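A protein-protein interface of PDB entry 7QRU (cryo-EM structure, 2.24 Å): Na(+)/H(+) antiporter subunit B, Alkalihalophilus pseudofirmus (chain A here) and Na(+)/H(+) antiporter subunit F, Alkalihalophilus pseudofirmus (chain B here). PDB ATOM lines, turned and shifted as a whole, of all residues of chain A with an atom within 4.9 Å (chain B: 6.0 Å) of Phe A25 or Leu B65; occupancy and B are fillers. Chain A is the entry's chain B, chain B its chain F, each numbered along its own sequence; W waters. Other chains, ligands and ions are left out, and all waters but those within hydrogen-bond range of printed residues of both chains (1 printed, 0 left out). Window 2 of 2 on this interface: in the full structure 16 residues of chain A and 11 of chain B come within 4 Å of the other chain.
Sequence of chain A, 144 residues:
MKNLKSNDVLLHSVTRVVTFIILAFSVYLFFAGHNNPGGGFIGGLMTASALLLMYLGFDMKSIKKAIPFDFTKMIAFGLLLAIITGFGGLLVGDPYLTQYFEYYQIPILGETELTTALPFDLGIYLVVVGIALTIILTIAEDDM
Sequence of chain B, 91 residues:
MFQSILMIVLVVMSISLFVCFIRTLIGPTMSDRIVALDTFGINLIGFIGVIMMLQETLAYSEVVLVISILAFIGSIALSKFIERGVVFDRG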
ATOM      1  N   ILE A  21     -11.158 -10.269   2.072  1.00  0.00           N
ATOM      2  CA  ILE A  21      -9.849 -10.055   2.655  1.00  0.00           C
ATOM      3  C   ILE A  21      -9.479  -8.588   2.592  1.00  0.00           C
ATOM      4  O   ILE A  21      -8.968  -8.077   3.611  1.00  0.00           O
ATOM      5  CB  ILE A  21      -8.793 -10.946   1.981  1.00  0.00           C
ATOM      6  CG1 ILE A  21      -9.107 -12.439   2.134  1.00  0.00           C
ATOM      7  CG2 ILE A  21      -7.432 -10.702   2.582  1.00  0.00           C
ATOM      8  CD1 ILE A  21      -8.369 -13.349   1.087  1.00  0.00           C
ATOM      9  N   ILE A  22      -9.679  -7.938   1.442  1.00  0.00           N
ATOM     10  CA  ILE A  22      -9.400  -6.523   1.395  1.00  0.00           C
ATOM     11  C   ILE A  22     -10.252  -5.754   2.394  1.00  0.00           C
ATOM     12  O   ILE A  22      -9.726  -4.874   3.060  1.00  0.00           O
ATOM     13  CB  ILE A  22      -9.510  -5.955  -0.007  1.00  0.00           C
ATOM     14  CG1 ILE A  22      -8.642  -6.790  -0.960  1.00  0.00           C
ATOM     15  CG2 ILE A  22      -9.000  -4.522  -0.028  1.00  0.00           C
ATOM     16  CD1 ILE A  22      -9.002  -6.562  -2.427  1.00  0.00           C
ATOM     17  N   LEU A  23     -11.548  -5.985   2.492  1.00  0.00           N
ATOM     18  CA  LEU A  23     -12.298  -5.237   3.471  1.00  0.00           C
ATOM     19  C   LEU A  23     -11.779  -5.459   4.896  1.00  0.00           C
ATOM     20  O   LEU A  23     -11.625  -4.510   5.686  1.00  0.00           O
ATOM     21  CB  LEU A  23     -13.719  -5.677   3.405  1.00  0.00           C
ATOM     22  CG  LEU A  23     -14.631  -4.938   2.472  1.00  0.00           C
ATOM     23  CD1 LEU A  23     -16.050  -5.489   2.652  1.00  0.00           C
ATOM     24  CD2 LEU A  23     -14.622  -3.475   2.789  1.00  0.00           C
ATOM     25  N   ALA A  24     -11.507  -6.703   5.262  1.00  0.00           N
ATOM     26  CA  ALA A  24     -10.997  -6.919   6.585  1.00  0.00           C
ATOM     27  C   ALA A  24      -9.695  -6.145   6.751  1.00  0.00           C
ATOM     28  O   ALA A  24      -9.409  -5.592   7.800  1.00  0.00           O
ATOM     29  CB  ALA A  24     -10.817  -8.392   6.839  1.00  0.00           C
ATOM     30  N   PHE A  25      -8.800  -6.182   5.768  1.00  0.00           N
ATOM     31  CA  PHE A  25      -7.558  -5.451   5.867  1.00  0.00           C
ATOM     32  C   PHE A  25      -7.826  -3.955   5.897  1.00  0.00           C
ATOM     33  O   PHE A  25      -7.147  -3.215   6.584  1.00  0.00           O
ATOM     34  CB  PHE A  25      -6.696  -5.896   4.693  1.00  0.00           C
ATOM     35  CG  PHE A  25      -5.337  -5.297   4.686  1.00  0.00           C
ATOM     36  CD1 PHE A  25      -4.538  -5.393   5.798  1.00  0.00           C
ATOM     37  CD2 PHE A  25      -4.849  -4.713   3.527  1.00  0.00           C
ATOM     38  CE1 PHE A  25      -3.278  -4.814   5.775  1.00  0.00           C
ATOM     39  CE2 PHE A  25      -3.537  -4.243   3.494  1.00  0.00           C
ATOM     40  CZ  PHE A  25      -2.790  -4.203   4.648  1.00  0.00           C
ATOM     41  N   SER A  26      -8.789  -3.447   5.159  1.00  0.00           N
ATOM     42  CA  SER A  26      -9.052  -2.011   5.295  1.00  0.00           C
ATOM     43  C   SER A  26      -9.513  -1.617   6.680  1.00  0.00           C
ATOM     44  O   SER A  26      -9.187  -0.532   7.099  1.00  0.00           O
ATOM     45  CB  SER A  26     -10.010  -1.585   4.294  1.00  0.00           C
ATOM     46  OG  SER A  26     -11.281  -2.031   4.634  1.00  0.00           O
ATOM     47  N   VAL A  27     -10.320  -2.422   7.348  1.00  0.00           N
ATOM     48  CA  VAL A  27     -10.702  -2.071   8.701  1.00  0.00           C
ATOM     49  C   VAL A  27      -9.496  -2.159   9.623  1.00  0.00           C
ATOM     50  O   VAL A  27      -9.383  -1.356  10.504  1.00  0.00           O
ATOM     51  CB  VAL A  27     -11.865  -2.941   9.206  1.00  0.00           C
ATOM     52  CG1 VAL A  27     -12.158  -2.688  10.655  1.00  0.00           C
ATOM     53  CG2 VAL A  27     -13.039  -2.761   8.310  1.00  0.00           C
ATOM     54  N   TYR A  28      -8.641  -3.157   9.494  1.00  0.00           N
ATOM     55  CA  TYR A  28      -7.447  -3.183  10.318  1.00  0.00           C
ATOM     56  C   TYR A  28      -6.619  -1.910  10.090  1.00  0.00           C
ATOM     57  O   TYR A  28      -6.067  -1.412  11.050  1.00  0.00           O
ATOM     58  CB  TYR A  28      -6.669  -4.465   9.950  1.00  0.00           C
ATOM     59  CG  TYR A  28      -5.244  -4.443  10.385  1.00  0.00           C
ATOM     60  CD1 TYR A  28      -4.934  -4.661  11.702  1.00  0.00           C
ATOM     61  CD2 TYR A  28      -4.249  -4.058   9.487  1.00  0.00           C
ATOM     62  CE1 TYR A  28      -3.639  -4.466  12.146  1.00  0.00           C
ATOM     63  CE2 TYR A  28      -2.948  -3.836   9.924  1.00  0.00           C
ATOM     64  CZ  TYR A  28      -2.662  -4.023  11.263  1.00  0.00           C
ATOM     65  OH  TYR A  28      -1.388  -3.796  11.725  1.00  0.00           O
ATOM     66  N   LEU A  29      -6.352  -1.497   8.847  1.00  0.00           N
ATOM     67  CA  LEU A  29      -5.583  -0.307   8.548  1.00  0.00           C
ATOM     68  C   LEU A  29      -6.208   0.903   9.214  1.00  0.00           C
ATOM     69  O   LEU A  29      -5.511   1.560   9.956  1.00  0.00           O
ATOM     70  CB  LEU A  29      -5.518  -0.125   7.036  1.00  0.00           C
ATOM     71  CG  LEU A  29      -4.542  -1.114   6.369  1.00  0.00           C
ATOM     72  CD1 LEU A  29      -4.714  -1.076   4.873  1.00  0.00           C
ATOM     73  CD2 LEU A  29      -3.142  -0.828   6.805  1.00  0.00           C
ATOM     74  N   MET A  46      -8.191   1.959   0.997  1.00  0.00           N
ATOM     75  CA  MET A  46      -8.223   0.513   0.918  1.00  0.00           C
ATOM     76  C   MET A  46      -9.618  -0.051   0.822  1.00  0.00           C
ATOM     77  O   MET A  46      -9.895  -0.940   0.003  1.00  0.00           O
ATOM     78  CB  MET A  46      -7.469  -0.103   2.064  1.00  0.00           C
ATOM     79  CG  MET A  46      -7.232  -1.629   1.950  1.00  0.00           C
ATOM     80  SD  MET A  46      -6.396  -2.115   0.448  1.00  0.00           S
ATOM     81  CE  MET A  46      -4.795  -1.453   0.741  1.00  0.00           C
ATOM     82  N   TYR B  60       7.230  -2.363   7.137  1.00  0.00           N
ATOM     83  CA  TYR B  60       6.750  -2.409   5.774  1.00  0.00           C
ATOM     84  C   TYR B  60       5.877  -3.591   5.505  1.00  0.00           C
ATOM     85  O   TYR B  60       5.496  -3.703   4.341  1.00  0.00           O
ATOM     86  CB  TYR B  60       7.884  -2.337   4.750  1.00  0.00           C
ATOM     87  CG  TYR B  60       8.850  -1.258   5.123  1.00  0.00           C
ATOM     88  CD1 TYR B  60       8.467   0.088   5.197  1.00  0.00           C
ATOM     89  CD2 TYR B  60      10.145  -1.576   5.387  1.00  0.00           C
ATOM     90  CE1 TYR B  60       9.353   1.085   5.593  1.00  0.00           C
ATOM     91  CE2 TYR B  60      11.047  -0.617   5.806  1.00  0.00           C
ATOM     92  CZ  TYR B  60      10.628   0.691   5.963  1.00  0.00           C
ATOM     93  OH  TYR B  60      11.567   1.531   6.377  1.00  0.00           O
ATOM     94  N   SER B  61       5.419  -4.348   6.490  1.00  0.00           N
ATOM     95  CA  SER B  61       4.622  -5.557   6.169  1.00  0.00           C
ATOM     96  C   SER B  61       3.251  -5.253   5.564  1.00  0.00           C
ATOM     97  O   SER B  61       2.859  -5.867   4.595  1.00  0.00           O
ATOM     98  CB  SER B  61       4.464  -6.407   7.364  1.00  0.00           C
ATOM     99  OG  SER B  61       4.143  -5.594   8.478  1.00  0.00           O
ATOM    100  N   GLU B  62       2.625  -4.129   5.907  1.00  0.00           N
ATOM    101  CA  GLU B  62       1.414  -3.697   5.207  1.00  0.00           C
ATOM    102  C   GLU B  62       1.675  -3.320   3.743  1.00  0.00           C
ATOM    103  O   GLU B  62       0.850  -3.593   2.891  1.00  0.00           O
ATOM    104  CB  GLU B  62       0.772  -2.476   5.877  1.00  0.00           C
ATOM    105  CG  GLU B  62       0.373  -2.818   7.305  1.00  0.00           C
ATOM    106  CD  GLU B  62       1.544  -2.800   8.318  1.00  0.00           C
ATOM    107  OE1 GLU B  62       2.638  -2.044   8.126  1.00  0.00           O
ATOM    108  OE2 GLU B  62       1.449  -3.618   9.295  1.00  0.00           O
ATOM    109  N   VAL B  63       2.807  -2.705   3.422  1.00  0.00           N
ATOM    110  CA  VAL B  63       3.117  -2.350   2.050  1.00  0.00           C
ATOM    111  C   VAL B  63       3.132  -3.557   1.123  1.00  0.00           C
ATOM    112  O   VAL B  63       2.558  -3.421   0.029  1.00  0.00           O
ATOM    113  CB  VAL B  63       4.437  -1.601   1.909  1.00  0.00           C
ATOM    114  CG1 VAL B  63       4.680  -1.196   0.496  1.00  0.00           C
ATOM    115  CG2 VAL B  63       4.475  -0.402   2.828  1.00  0.00           C
ATOM    116  N   VAL B  64       3.587  -4.740   1.555  1.00  0.00           N
ATOM    117  CA  VAL B  64       3.718  -5.815   0.577  1.00  0.00           C
ATOM    118  C   VAL B  64       2.321  -6.285   0.261  1.00  0.00           C
ATOM    119  O   VAL B  64       2.025  -6.556  -0.894  1.00  0.00           O
ATOM    120  CB  VAL B  64       4.663  -6.979   0.955  1.00  0.00           C
ATOM    121  CG1 VAL B  64       6.121  -6.525   0.982  1.00  0.00           C
ATOM    122  CG2 VAL B  64       4.346  -7.545   2.253  1.00  0.00           C
ATOM    123  N   LEU B  65       1.456  -6.303   1.272  1.00  0.00           N
ATOM    124  CA  LEU B  65       0.106  -6.769   1.084  1.00  0.00           C
ATOM    125  C   LEU B  65      -0.672  -5.786   0.227  1.00  0.00           C
ATOM    126  O   LEU B  65      -1.306  -6.167  -0.750  1.00  0.00           O
ATOM    127  CB  LEU B  65      -0.462  -6.975   2.479  1.00  0.00           C
ATOM    128  CG  LEU B  65      -1.898  -7.492   2.563  1.00  0.00           C
ATOM    129  CD1 LEU B  65      -2.168  -8.684   1.633  1.00  0.00           C
ATOM    130  CD2 LEU B  65      -2.148  -7.863   4.020  1.00  0.00           C
ATOM    131  N   VAL B  66      -0.455  -4.477   0.376  1.00  0.00           N
ATOM    132  CA  VAL B  66      -1.135  -3.526  -0.515  1.00  0.00           C
ATOM    133  C   VAL B  66      -0.640  -3.710  -1.950  1.00  0.00           C
ATOM    134  O   VAL B  66      -1.411  -3.538  -2.880  1.00  0.00           O
ATOM    135  CB  VAL B  66      -0.918  -2.080  -0.004  1.00  0.00           C
ATOM    136  CG1 VAL B  66      -1.434  -1.000  -0.913  1.00  0.00           C
ATOM    137  CG2 VAL B  66      -1.556  -1.884   1.354  1.00  0.00           C
ATOM    138  N   ILE B  67       0.656  -3.922  -2.178  1.00  0.00           N
ATOM    139  CA  ILE B  67       1.139  -3.997  -3.540  1.00  0.00           C
ATOM    140  C   ILE B  67       0.478  -5.188  -4.210  1.00  0.00           C
ATOM    141  O   ILE B  67       0.116  -5.125  -5.359  1.00  0.00           O
ATOM    142  CB  ILE B  67       2.670  -4.126  -3.610  1.00  0.00           C
ATOM    143  CG1 ILE B  67       3.359  -2.855  -3.222  1.00  0.00           C
ATOM    144  CG2 ILE B  67       3.112  -4.620  -4.978  1.00  0.00           C
ATOM    145  CD1 ILE B  67       4.782  -3.123  -2.890  1.00  0.00           C
ATOM    146  N   SER B  68       0.426  -6.320  -3.536  1.00  0.00           N
ATOM    147  CA  SER B  68      -0.187  -7.471  -4.169  1.00  0.00           C
ATOM    148  C   SER B  68      -1.640  -7.157  -4.585  1.00  0.00           C
ATOM    149  O   SER B  68      -2.037  -7.447  -5.687  1.00  0.00           O
ATOM    150  CB  SER B  68      -0.044  -8.625  -3.220  1.00  0.00           C
ATOM    151  OG  SER B  68      -1.018  -8.583  -2.207  1.00  0.00           O
ATOM    152  N   ILE B  69      -2.426  -6.470  -3.738  1.00  0.00           N
ATOM    153  CA  ILE B  69      -3.788  -6.107  -4.070  1.00  0.00           C
ATOM    154  C   ILE B  69      -3.784  -5.147  -5.248  1.00  0.00           C
ATOM    155  O   ILE B  69      -4.559  -5.293  -6.181  1.00  0.00           O
ATOM    156  CB  ILE B  69      -4.561  -5.570  -2.854  1.00  0.00           C
ATOM    157  CG1 ILE B  69      -4.781  -6.687  -1.834  1.00  0.00           C
ATOM    158  CG2 ILE B  69      -5.878  -4.931  -3.216  1.00  0.00           C
ATOM    159  CD1 ILE B  69      -4.834  -6.061  -0.361  1.00  0.00           C
ATOM    160  N   LEU B  70      -2.997  -4.128  -5.199  1.00  0.00           N
ATOM    161  CA  LEU B  70      -3.090  -3.125  -6.247  1.00  0.00           C
ATOM    162  C   LEU B  70      -2.560  -3.609  -7.586  1.00  0.00           C
ATOM    163  O   LEU B  70      -3.076  -3.156  -8.603  1.00  0.00           O
ATOM    164  CB  LEU B  70      -2.339  -1.873  -5.728  1.00  0.00           C
ATOM    165  CG  LEU B  70      -3.109  -1.271  -4.494  1.00  0.00           C
ATOM    166  CD1 LEU B  70      -2.510   0.001  -3.962  1.00  0.00           C
ATOM    167  CD2 LEU B  70      -4.630  -0.995  -4.753  1.00  0.00           C
HETATM  168  O   HOH W   1      -0.245  -1.452  10.362  1.00  0.00           O
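The backbone carbonyl oxygen (O) of Leu B65 lies within hydrogen-bond range of the side-chain hydroxyl (OG) of Ser B68, 2.8 Å away.
OE2 of Glu B62 lies within hydrogen-bond range of OG of Ser B61 (3.4 Å).
Among the printed residues, pairs that only touch across the chains: Ile A22 with Ile B69 (3.6 Å), Phe A25 with Leu B65 (3.7 Å), Phe A25 with Val B66 (3.8 Å), Tyr A28 with Glu B62 (3.7 Å) and Met A46 with Val B66 (3.3 Å).
Phe A25 touches just these residues of chain B: Leu B65 and Val B66.
Of the printed residues of chain A, Leu B65 touches Phe A25 (3.7 Å).
Printed residues of chain A within 4 Å of Val B66: Phe A25 and Met A46.
Printed residues of chain B within 4 Å of Tyr A28: Glu B62.
Of the printed residues of chain A, Glu B62 touches Tyr A28.
Of the printed residues of chain A, Ile B69 touches Ile A22.
Leu A29 touches none of the printed residues of chain B.
The nearest printed residue of chain B that does not touch Met A46 is Ile B69 (4.3 Å).
Of the 10 printed residues of chain A, 4 touch a printed residue of chain B.
Hydrophobic or aromatic side chains of chain A within 4 Å of the printed part of chain B: Ile A22, Phe A25, Tyr A28 and Met A46.
Of the 11 printed residues of chain B, 4 touch a printed residue of chain A.
Hydrophobic or aromatic side chains of chain B that line the printed part of chain A: Leu B65, Val B66 and Ile B69.
Among the printed residues, 5 pairs touch across the chains.
Among the printed residues, no Asp or Glu carboxylate lies within 4 Å of a Lys or Arg side-chain nitrogen of the other chain.
Water W1 lies within hydrogen-bond range of OH of Tyr A28 (2.9 Å) and OE2 of Glu B62 (2.9 Å).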
